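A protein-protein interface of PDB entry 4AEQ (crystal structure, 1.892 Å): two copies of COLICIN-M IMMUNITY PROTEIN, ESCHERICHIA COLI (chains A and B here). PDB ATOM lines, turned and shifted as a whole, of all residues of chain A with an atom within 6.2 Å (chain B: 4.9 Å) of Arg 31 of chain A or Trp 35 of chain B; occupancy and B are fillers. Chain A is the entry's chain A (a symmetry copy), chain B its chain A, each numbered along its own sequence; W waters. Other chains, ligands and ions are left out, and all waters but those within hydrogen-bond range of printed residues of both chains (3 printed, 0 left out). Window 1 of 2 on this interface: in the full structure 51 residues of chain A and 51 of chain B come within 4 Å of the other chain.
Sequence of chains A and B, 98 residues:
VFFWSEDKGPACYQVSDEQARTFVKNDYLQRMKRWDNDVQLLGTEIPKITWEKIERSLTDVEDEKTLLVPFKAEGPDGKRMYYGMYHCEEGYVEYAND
O of Val 93 of chain A sits at hydrogen-bond distance from NH2 of Arg 31 of chain B (2.7 Å). NH2 of Arg 31 of chain A lies within hydrogen-bond range of O of Val 93 of chain B, at 2.7 Å. OH of Tyr 95 of chain B is in hydrogen-bond range of OD2 of Asp 27 of chain A, at 2.6 Å. N of Tyr 28 of chain A sits at hydrogen-bond distance from OH of Tyr 95 of chain B (3.0 Å). The side-chain carboxylate (OE2) of Glu 45 of chain A lies close to the side-chain amide oxygen (OD1) of Asn 37 of chain B, 2.7 Å away. The side-chain carboxylate (OE2) of Glu 45 of chain A sits close to the side-chain carboxylate (OD2) of Asp 36 of chain B, at 2.6 Å. OD1 of Asp 36 of chain A lies close to OD1 of Asp 36 of chain B (3.1 Å).
O of Lys 33 of chain B lies close to OD1 of Asn 37 of chain B. The side-chain amide nitrogen (NE2) of Gln 30 of chain A sits at hydrogen-bond distance from the side-chain carboxylate (OD1) of Asp 27 of chain A, 3.4 Å away. The side-chain sulfur (SD) of Met 32 of chain A sits at hydrogen-bond distance from the side-chain hydroxyl (OH) of Tyr 28 of chain A, 3.6 Å away. The guanidinium group (NE) of Arg 31 of chain A is in salt-bridge range of the side-chain carboxylate (OD2) of Asp 27 of chain A, 3.1 Å away.
Val 93 of chain B touches Asp 27 of chain A. Tyr 28 of chain A touches Trp 35 of chain B (CE1 to CZ3, 3.5 Å). Trp 35 of chain B touches Arg 31 of chain A (CZ2 to CD, 3.5 Å). Arg 31 of chain A touches Tyr 95 of chain B (NH1 to CE1, 3.2 Å). Met 32 of chain A touches Trp 35 of chain B. CG2 of Val 39 of chain B touches CE of Met 32 of chain A (3.6 Å). CD of Arg 31 of chain B touches CZ2 of Trp 35 of chain A (3.5 Å). Asp 36 of chain A touches Val 39 of chain B. Glu 45 of chain A touches Met 32 of chain B. Lys 33 of chain B touches Glu 45 of chain A.
Arg 31 of chain A touches just these residues of chain B: Trp 35, Val 93 and Tyr 95. Of chain A, only Tyr 28 (3.5 Å), Arg 31 (3.5 Å), Met 32 (3.6 Å) and Trp 35 (3.3 Å) come within 4 Å of Trp 35 of chain B. Of the printed residues of chain A, Val 93 of chain B touches Asp 27 (3.7 Å) and Arg 31 (2.7 Å). Of the printed residues of chain A, Val 39 of chain B touches Met 32 (3.6 Å) and Asp 36 (3.7 Å). Of the printed residues of chain B, Glu 45 of chain A touches Met 32, Lys 33, Asp 36 and Asn 37. Printed residues of chain B within 4 Å of Trp 35 of chain A: Arg 31, Met 32 and Trp 35. Arg 34 of chain A touches none of the printed residues of chain B. The nearest residue of chain B that does not touch Arg 31 of chain A is Glu 94 of chain B (4.5 Å).
Printed residues of chain A that touch a printed residue of chain B: Asp 27, Tyr 28, Arg 31, Met 32, Trp 35, Asp 36, Glu 45 and Val 93. Hydrophobic or aromatic side chains of chain A that line the printed part of chain B: Tyr 28, Met 32 and Trp 35. Along chain A the printed residues that touch a printed residue of chain B span positions 27 to 93.
Arg 31 of chain A touches Trp 35 of chain B, and with the chains exchanged Trp 35 of chain A touches Arg 31 of chain B. Arg 31 of chain A touches Val 93 of chain B, and with the chains exchanged Val 93 of chain A touches Arg 31 of chain B. Met 32 of chain A touches Trp 35 of chain B, and with the chains exchanged Trp 35 of chain A touches Met 32 of chain B. Asp 36 of chain A touches its own counterpart, Asp 36 of chain B. 7 positions are printed for both chains. Of the 19 pairs that touch across the chains among the printed residues, 8 have their exchanged pair printed and touching as well.
Water W2 lies within hydrogen-bond range of the side-chain carboxylate (OD1) of Asp 27 of chain A, the guanidinium group (NH2) of Arg 31 of chain A and the backbone NH (N) of Val 93 of chain B. Water W3 bridges NH2 of Arg 31 of chain B (2.6 Å) and N of Val 93 of chain A (2.8 Å). Water W1 lies within hydrogen-bond range of the guanidinium group of Arg 31 of chain A and the guanidinium group of Arg 31 of chain B.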
ATOM      1  N   ASN A  26      33.817  11.408   8.797  1.00  0.00           N
ATOM      2  CA  ASN A  26      33.624  12.858   8.783  1.00  0.00           C
ATOM      3  C   ASN A  26      32.376  13.238   9.567  1.00  0.00           C
ATOM      4  O   ASN A  26      32.407  14.110  10.447  1.00  0.00           O
ATOM      5  CB  ASN A  26      33.512  13.389   7.349  1.00  0.00           C
ATOM      6  CG  ASN A  26      34.852  13.446   6.638  1.00  0.00           C
ATOM      7  OD1 ASN A  26      35.907  13.362   7.267  1.00  0.00           O
ATOM      8  ND2 ASN A  26      34.813  13.609   5.323  1.00  0.00           N
ATOM      9  N   ASP A  27      31.278  12.569   9.239  1.00  0.00           N
ATOM     10  CA  ASP A  27      29.988  12.848   9.858  1.00  0.00           C
ATOM     11  C   ASP A  27      30.006  12.609  11.367  1.00  0.00           C
ATOM     12  O   ASP A  27      29.533  13.440  12.151  1.00  0.00           O
ATOM     13  CB  ASP A  27      28.913  11.988   9.196  1.00  0.00           C
ATOM     14  CG  ASP A  27      27.533  12.278   9.723  1.00  0.00           C
ATOM     15  OD1 ASP A  27      26.886  13.209   9.205  1.00  0.00           O
ATOM     16  OD2 ASP A  27      27.095  11.573  10.651  1.00  0.00           O
ATOM     17  N   TYR A  28      30.550  11.465  11.770  1.00  0.00           N
ATOM     18  CA  TYR A  28      30.610  11.093  13.178  1.00  0.00           C
ATOM     19  C   TYR A  28      31.417  12.100  13.989  1.00  0.00           C
ATOM     20  O   TYR A  28      30.952  12.596  15.020  1.00  0.00           O
ATOM     21  CB  TYR A  28      31.206   9.694  13.338  1.00  0.00           C
ATOM     22  CG  TYR A  28      31.458   9.300  14.776  1.00  0.00           C
ATOM     23  CD1 TYR A  28      30.431   8.816  15.576  1.00  0.00           C
ATOM     24  CD2 TYR A  28      32.725   9.416  15.333  1.00  0.00           C
ATOM     25  CE1 TYR A  28      30.663   8.454  16.893  1.00  0.00           C
ATOM     26  CE2 TYR A  28      32.965   9.057  16.645  1.00  0.00           C
ATOM     27  CZ  TYR A  28      31.936   8.576  17.419  1.00  0.00           C
ATOM     28  OH  TYR A  28      32.183   8.220  18.725  1.00  0.00           O
ATOM     29  N   LEU A  29      32.627  12.398  13.529  1.00  0.00           N
ATOM     30  CA  LEU A  29      33.473  13.358  14.240  1.00  0.00           C
ATOM     31  C   LEU A  29      32.835  14.749  14.313  1.00  0.00           C
ATOM     32  O   LEU A  29      32.831  15.397  15.374  1.00  0.00           O
ATOM     33  CB  LEU A  29      34.871  13.423  13.616  1.00  0.00           C
ATOM     34  CG  LEU A  29      35.725  12.171  13.846  1.00  0.00           C
ATOM     35  CD1 LEU A  29      37.082  12.308  13.171  1.00  0.00           C
ATOM     36  CD2 LEU A  29      35.888  11.879  15.344  1.00  0.00           C
ATOM     37  N   GLN A  30      32.288  15.206  13.188  1.00  0.00           N
ATOM     38  CA  GLN A  30      31.644  16.514  13.162  1.00  0.00           C
ATOM     39  C   GLN A  30      30.498  16.560  14.169  1.00  0.00           C
ATOM     40  O   GLN A  30      30.341  17.545  14.890  1.00  0.00           O
ATOM     41  CB  GLN A  30      31.134  16.856  11.757  1.00  0.00           C
ATOM     42  CG  GLN A  30      29.676  16.497  11.529  1.00  0.00           C
ATOM     43  CD  GLN A  30      29.192  16.852  10.137  1.00  0.00           C
ATOM     44  OE1 GLN A  30      29.893  17.515   9.369  1.00  0.00           O
ATOM     45  NE2 GLN A  30      27.982  16.414   9.806  1.00  0.00           N
ATOM     46  N   ARG A  31      29.702  15.495  14.225  1.00  0.00           N
ATOM     47  CA  ARG A  31      28.582  15.435  15.159  1.00  0.00           C
ATOM     48  C   ARG A  31      29.027  15.444  16.615  1.00  0.00           C
ATOM     49  O   ARG A  31      28.500  16.200  17.430  1.00  0.00           O
ATOM     50  CB  ARG A  31      27.717  14.210  14.879  1.00  0.00           C
ATOM     51  CG  ARG A  31      26.941  14.297  13.585  1.00  0.00           C
ATOM     52  CD  ARG A  31      25.950  13.161  13.471  1.00  0.00           C
ATOM     53  NE  ARG A  31      25.117  13.276  12.278  1.00  0.00           N
ATOM     54  CZ  ARG A  31      24.135  12.441  11.968  1.00  0.00           C
ATOM     55  NH1 ARG A  31      23.851  11.427  12.766  1.00  0.00           N
ATOM     56  NH2 ARG A  31      23.431  12.626  10.865  1.00  0.00           N
ATOM     57  N   MET A  32      30.004  14.605  16.937  1.00  0.00           N
ATOM     58  CA  MET A  32      30.551  14.577  18.286  1.00  0.00           C
ATOM     59  C   MET A  32      30.930  15.990  18.707  1.00  0.00           C
ATOM     60  O   MET A  32      30.484  16.489  19.758  1.00  0.00           O
ATOM     61  CB  MET A  32      31.780  13.669  18.349  1.00  0.00           C
ATOM     62  CG  MET A  32      31.456  12.190  18.205  1.00  0.00           C
ATOM     63  SD  MET A  32      31.063  11.417  19.789  1.00  0.00           S
ATOM     64  CE  MET A  32      32.696  11.343  20.519  1.00  0.00           C
ATOM     65  N   LYS A  33      31.734  16.641  17.866  1.00  0.00           N
ATOM     66  CA  LYS A  33      32.171  18.009  18.132  1.00  0.00           C
ATOM     67  C   LYS A  33      31.001  18.971  18.342  1.00  0.00           C
ATOM     68  O   LYS A  33      30.913  19.642  19.373  1.00  0.00           O
ATOM     69  CB  LYS A  33      33.042  18.512  16.981  1.00  0.00           C
ATOM     70  CG  LYS A  33      33.338  20.004  17.028  1.00  0.00           C
ATOM     71  CD  LYS A  33      34.266  20.392  15.890  1.00  0.00           C
ATOM     72  CE  LYS A  33      35.547  19.571  15.944  1.00  0.00           C
ATOM     73  NZ  LYS A  33      36.292  19.601  14.656  1.00  0.00           N
ATOM     74  N   ARG A  34      30.107  19.039  17.363  1.00  0.00           N
ATOM     75  CA  ARG A  34      28.994  19.983  17.406  1.00  0.00           C
ATOM     76  C   ARG A  34      28.103  19.829  18.629  1.00  0.00           C
ATOM     77  O   ARG A  34      27.850  20.792  19.351  1.00  0.00           O
ATOM     78  CB  ARG A  34      28.149  19.862  16.140  1.00  0.00           C
ATOM     79  CG  ARG A  34      28.788  20.480  14.917  1.00  0.00           C
ATOM     80  CD  ARG A  34      27.961  20.224  13.683  1.00  0.00           C
ATOM     81  NE  ARG A  34      28.630  20.699  12.479  1.00  0.00           N
ATOM     82  CZ  ARG A  34      28.521  20.116  11.292  1.00  0.00           C
ATOM     83  NH1 ARG A  34      27.770  19.036  11.155  1.00  0.00           N
ATOM     84  NH2 ARG A  34      29.165  20.606  10.246  1.00  0.00           N
ATOM     85  N   TRP A  35      27.624  18.612  18.856  1.00  0.00           N
ATOM     86  CA  TRP A  35      26.691  18.382  19.954  1.00  0.00           C
ATOM     87  C   TRP A  35      27.349  18.564  21.321  1.00  0.00           C
ATOM     88  O   TRP A  35      26.761  19.189  22.218  1.00  0.00           O
ATOM     89  CB  TRP A  35      26.002  17.020  19.819  1.00  0.00           C
ATOM     90  CG  TRP A  35      25.120  16.964  18.612  1.00  0.00           C
ATOM     91  CD1 TRP A  35      25.360  16.293  17.450  1.00  0.00           C
ATOM     92  CD2 TRP A  35      23.861  17.626  18.440  1.00  0.00           C
ATOM     93  NE1 TRP A  35      24.323  16.488  16.567  1.00  0.00           N
ATOM     94  CE2 TRP A  35      23.391  17.303  17.153  1.00  0.00           C
ATOM     95  CE3 TRP A  35      23.086  18.456  19.254  1.00  0.00           C
ATOM     96  CZ2 TRP A  35      22.180  17.780  16.660  1.00  0.00           C
ATOM     97  CZ3 TRP A  35      21.884  18.929  18.763  1.00  0.00           C
ATOM     98  CH2 TRP A  35      21.441  18.589  17.478  1.00  0.00           C
ATOM     99  N   ASP A  36      28.570  18.050  21.483  1.00  0.00           N
ATOM    100  CA  ASP A  36      29.271  18.281  22.744  1.00  0.00           C
ATOM    101  C   ASP A  36      29.435  19.776  22.999  1.00  0.00           C
ATOM    102  O   ASP A  36      29.168  20.271  24.102  1.00  0.00           O
ATOM    103  CB  ASP A  36      30.640  17.609  22.765  1.00  0.00           C
ATOM    104  CG  ASP A  36      31.315  17.729  24.119  1.00  0.00           C
ATOM    105  OD1 ASP A  36      30.698  17.309  25.123  1.00  0.00           O
ATOM    106  OD2 ASP A  36      32.443  18.260  24.187  1.00  0.00           O
ATOM    107  N   GLU A  45      22.182  19.403  29.126  1.00  0.00           N
ATOM    108  CA  GLU A  45      21.776  18.468  28.081  1.00  0.00           C
ATOM    109  C   GLU A  45      20.315  18.675  27.708  1.00  0.00           C
ATOM    110  O   GLU A  45      19.862  18.236  26.651  1.00  0.00           O
ATOM    111  CB  GLU A  45      21.971  17.021  28.545  1.00  0.00           C
ATOM    112  CG  GLU A  45      23.316  16.416  28.191  1.00  0.00           C
ATOM    113  CD  GLU A  45      23.393  14.943  28.541  1.00  0.00           C
ATOM    114  OE1 GLU A  45      22.433  14.428  29.156  1.00  0.00           O
ATOM    115  OE2 GLU A  45      24.407  14.299  28.201  1.00  0.00           O
ATOM    116  N   VAL A  93      16.069  14.864  10.796  1.00  0.00           N
ATOM    117  CA  VAL A  93      16.246  16.307  10.847  1.00  0.00           C
ATOM    118  C   VAL A  93      17.726  16.586  10.711  1.00  0.00           C
ATOM    119  O   VAL A  93      18.546  15.851  11.265  1.00  0.00           O
ATOM    120  CB  VAL A  93      15.812  16.868  12.211  1.00  0.00           C
ATOM    121  CG1 VAL A  93      15.949  18.388  12.238  1.00  0.00           C
ATOM    122  CG2 VAL A  93      14.393  16.434  12.542  1.00  0.00           C
ATOM    123  N   ARG B  31      19.422  13.783  20.497  1.00  0.00           N
ATOM    124  CA  ARG B  31      20.774  13.950  19.971  1.00  0.00           C
ATOM    125  C   ARG B  31      21.725  14.582  20.978  1.00  0.00           C
ATOM    126  O   ARG B  31      22.834  14.095  21.190  1.00  0.00           O
ATOM    127  CB  ARG B  31      20.750  14.766  18.682  1.00  0.00           C
ATOM    128  CG  ARG B  31      20.130  14.036  17.514  1.00  0.00           C
ATOM    129  CD  ARG B  31      20.328  14.807  16.228  1.00  0.00           C
ATOM    130  NE  ARG B  31      19.826  14.078  15.067  1.00  0.00           N
ATOM    131  CZ  ARG B  31      19.925  14.506  13.816  1.00  0.00           C
ATOM    132  NH1 ARG B  31      20.512  15.660  13.554  1.00  0.00           N
ATOM    133  NH2 ARG B  31      19.442  13.775  12.826  1.00  0.00           N
ATOM    134  N   MET B  32      21.283  15.668  21.602  1.00  0.00           N
ATOM    135  CA  MET B  32      22.084  16.318  22.630  1.00  0.00           C
ATOM    136  C   MET B  32      22.525  15.281  23.656  1.00  0.00           C
ATOM    137  O   MET B  32      23.728  15.130  23.942  1.00  0.00           O
ATOM    138  CB  MET B  32      21.281  17.421  23.320  1.00  0.00           C
ATOM    139  CG  MET B  32      21.024  18.632  22.437  1.00  0.00           C
ATOM    140  SD  MET B  32      22.362  19.841  22.523  1.00  0.00           S
ATOM    141  CE  MET B  32      22.064  20.528  24.149  1.00  0.00           C
ATOM    142  N   LYS B  33      21.544  14.550  24.186  1.00  0.00           N
ATOM    143  CA  LYS B  33      21.817  13.507  25.173  1.00  0.00           C
ATOM    144  C   LYS B  33      22.823  12.470  24.672  1.00  0.00           C
ATOM    145  O   LYS B  33      23.854  12.233  25.306  1.00  0.00           O
ATOM    146  CB  LYS B  33      20.517  12.807  25.567  1.00  0.00           C
ATOM    147  CG  LYS B  33      20.714  11.542  26.389  1.00  0.00           C
ATOM    148  CD  LYS B  33      19.369  10.962  26.792  1.00  0.00           C
ATOM    149  CE  LYS B  33      18.549  11.995  27.553  1.00  0.00           C
ATOM    150  NZ  LYS B  33      17.105  11.643  27.605  1.00  0.00           N
ATOM    151  N   ARG B  34      22.519  11.850  23.538  1.00  0.00           N
ATOM    152  CA  ARG B  34      23.353  10.779  23.003  1.00  0.00           C
ATOM    153  C   ARG B  34      24.798  11.187  22.756  1.00  0.00           C
ATOM    154  O   ARG B  34      25.727  10.536  23.229  1.00  0.00           O
ATOM    155  CB  ARG B  34      22.749  10.232  21.711  1.00  0.00           C
ATOM    156  CG  ARG B  34      21.539   9.352  21.927  1.00  0.00           C
ATOM    157  CD  ARG B  34      20.923   8.943  20.613  1.00  0.00           C
ATOM    158  NE  ARG B  34      19.681   8.205  20.809  1.00  0.00           N
ATOM    159  CZ  ARG B  34      18.648   8.263  19.978  1.00  0.00           C
ATOM    160  NH1 ARG B  34      18.710   9.025  18.900  1.00  0.00           N
ATOM    161  NH2 ARG B  34      17.552   7.565  20.228  1.00  0.00           N
ATOM    162  N   TRP B  35      24.981  12.268  22.008  1.00  0.00           N
ATOM    163  CA  TRP B  35      26.330  12.690  21.644  1.00  0.00           C
ATOM    164  C   TRP B  35      27.130  13.178  22.850  1.00  0.00           C
ATOM    165  O   TRP B  35      28.312  12.827  22.998  1.00  0.00           O
ATOM    166  CB  TRP B  35      26.300  13.720  20.511  1.00  0.00           C
ATOM    167  CG  TRP B  35      25.777  13.130  19.240  1.00  0.00           C
ATOM    168  CD1 TRP B  35      24.557  13.350  18.672  1.00  0.00           C
ATOM    169  CD2 TRP B  35      26.456  12.201  18.385  1.00  0.00           C
ATOM    170  NE1 TRP B  35      24.437  12.623  17.511  1.00  0.00           N
ATOM    171  CE2 TRP B  35      25.589  11.909  17.314  1.00  0.00           C
ATOM    172  CE3 TRP B  35      27.712  11.593  18.422  1.00  0.00           C
ATOM    173  CZ2 TRP B  35      25.940  11.035  16.289  1.00  0.00           C
ATOM    174  CZ3 TRP B  35      28.059  10.725  17.403  1.00  0.00           C
ATOM    175  CH2 TRP B  35      27.176  10.455  16.350  1.00  0.00           C
ATOM    176  N   ASP B  36      26.496  13.962  23.724  1.00  0.00           N
ATOM    177  CA  ASP B  36      27.197  14.377  24.937  1.00  0.00           C
ATOM    178  C   ASP B  36      27.635  13.159  25.745  1.00  0.00           C
ATOM    179  O   ASP B  36      28.784  13.070  26.198  1.00  0.00           O
ATOM    180  CB  ASP B  36      26.336  15.283  25.811  1.00  0.00           C
ATOM    181  CG  ASP B  36      27.103  15.827  27.003  1.00  0.00           C
ATOM    182  OD1 ASP B  36      28.164  16.451  26.783  1.00  0.00           O
ATOM    183  OD2 ASP B  36      26.665  15.613  28.152  1.00  0.00           O
ATOM    184  N   ASN B  37      26.711  12.221  25.928  1.00  0.00           N
ATOM    185  CA  ASN B  37      27.035  11.009  26.659  1.00  0.00           C
ATOM    186  C   ASN B  37      28.224  10.288  26.038  1.00  0.00           C
ATOM    187  O   ASN B  37      29.173   9.953  26.739  1.00  0.00           O
ATOM    188  CB  ASN B  37      25.822  10.088  26.783  1.00  0.00           C
ATOM    189  CG  ASN B  37      24.798  10.610  27.774  1.00  0.00           C
ATOM    190  OD1 ASN B  37      24.965  11.688  28.351  1.00  0.00           O
ATOM    191  ND2 ASN B  37      23.727   9.852  27.971  1.00  0.00           N
ATOM    192  N   ASP B  38      28.194  10.063  24.728  1.00  0.00           N
ATOM    193  CA  ASP B  38      29.317   9.390  24.073  1.00  0.00           C
ATOM    194  C   ASP B  38      30.648  10.109  24.294  1.00  0.00           C
ATOM    195  O   ASP B  38      31.678   9.465  24.518  1.00  0.00           O
ATOM    196  CB  ASP B  38      29.046   9.171  22.579  1.00  0.00           C
ATOM    197  CG  ASP B  38      28.203   7.933  22.317  1.00  0.00           C
ATOM    198  OD1 ASP B  38      27.763   7.299  23.299  1.00  0.00           O
ATOM    199  OD2 ASP B  38      27.979   7.595  21.135  1.00  0.00           O
ATOM    200  N   VAL B  39      30.633  11.438  24.241  1.00  0.00           N
ATOM    201  CA  VAL B  39      31.870  12.181  24.472  1.00  0.00           C
ATOM    202  C   VAL B  39      32.376  11.977  25.899  1.00  0.00           C
ATOM    203  O   VAL B  39      33.552  11.673  26.109  1.00  0.00           O
ATOM    204  CB  VAL B  39      31.707  13.688  24.188  1.00  0.00           C
ATOM    205  CG1 VAL B  39      32.940  14.451  24.654  1.00  0.00           C
ATOM    206  CG2 VAL B  39      31.464  13.924  22.711  1.00  0.00           C
ATOM    207  N   TYR B  92      23.132  11.537   4.334  1.00  0.00           N
ATOM    208  CA  TYR B  92      23.150  11.572   5.791  1.00  0.00           C
ATOM    209  C   TYR B  92      23.382  10.189   6.377  1.00  0.00           C
ATOM    210  O   TYR B  92      23.170   9.174   5.712  1.00  0.00           O
ATOM    211  CB  TYR B  92      21.864  12.182   6.352  1.00  0.00           C
ATOM    212  CG  TYR B  92      20.667  11.258   6.340  1.00  0.00           C
ATOM    213  CD1 TYR B  92      19.888  11.118   5.203  1.00  0.00           C
ATOM    214  CD2 TYR B  92      20.306  10.544   7.472  1.00  0.00           C
ATOM    215  CE1 TYR B  92      18.791  10.288   5.189  1.00  0.00           C
ATOM    216  CE2 TYR B  92      19.208   9.708   7.470  1.00  0.00           C
ATOM    217  CZ  TYR B  92      18.455   9.585   6.323  1.00  0.00           C
ATOM    218  OH  TYR B  92      17.357   8.757   6.296  1.00  0.00           O
ATOM    219  N   VAL B  93      23.819  10.163   7.630  1.00  0.00           N
ATOM    220  CA  VAL B  93      24.074   8.919   8.338  1.00  0.00           C
ATOM    221  C   VAL B  93      23.226   8.931   9.591  1.00  0.00           C
ATOM    222  O   VAL B  93      23.081   9.977  10.227  1.00  0.00           O
ATOM    223  CB  VAL B  93      25.539   8.833   8.793  1.00  0.00           C
ATOM    224  CG1 VAL B  93      25.811   7.501   9.489  1.00  0.00           C
ATOM    225  CG2 VAL B  93      26.480   9.046   7.619  1.00  0.00           C
ATOM    226  N   GLU B  94      22.656   7.783   9.946  1.00  0.00           N
ATOM    227  CA  GLU B  94      22.014   7.663  11.261  1.00  0.00           C
ATOM    228  C   GLU B  94      22.708   6.548  12.009  1.00  0.00           C
ATOM    229  O   GLU B  94      23.046   5.529  11.424  1.00  0.00           O
ATOM    230  CB  GLU B  94      20.510   7.386  11.182  1.00  0.00           C
ATOM    231  CG  GLU B  94      20.191   6.063  10.576  1.00  0.00           C
ATOM    232  CD  GLU B  94      20.642   6.004   9.141  1.00  0.00           C
ATOM    233  OE1 GLU B  94      20.827   7.073   8.503  1.00  0.00           O
ATOM    234  OE2 GLU B  94      20.824   4.882   8.640  1.00  0.00           O
ATOM    235  N   TYR B  95      22.938   6.750  13.298  1.00  0.00           N
ATOM    236  CA  TYR B  95      23.769   5.831  14.063  1.00  0.00           C
ATOM    237  C   TYR B  95      22.967   4.936  14.993  1.00  0.00           C
ATOM    238  O   TYR B  95      21.977   5.359  15.586  1.00  0.00           O
ATOM    239  CB  TYR B  95      24.839   6.606  14.839  1.00  0.00           C
ATOM    240  CG  TYR B  95      25.785   7.364  13.935  1.00  0.00           C
ATOM    241  CD1 TYR B  95      25.487   8.649  13.508  1.00  0.00           C
ATOM    242  CD2 TYR B  95      26.968   6.788  13.498  1.00  0.00           C
ATOM    243  CE1 TYR B  95      26.341   9.344  12.673  1.00  0.00           C
ATOM    244  CE2 TYR B  95      27.832   7.475  12.660  1.00  0.00           C
ATOM    245  CZ  TYR B  95      27.511   8.756  12.253  1.00  0.00           C
ATOM    246  OH  TYR B  95      28.356   9.447  11.416  1.00  0.00           O
HETATM  247  O   HOH W   1      22.776  13.817  14.210  1.00  0.00           O
HETATM  248  O   HOH W   2      24.486  12.772   8.503  1.00  0.00           O
HETATM  249  O   HOH W   3      16.978  12.981  12.703  1.00  0.00           O
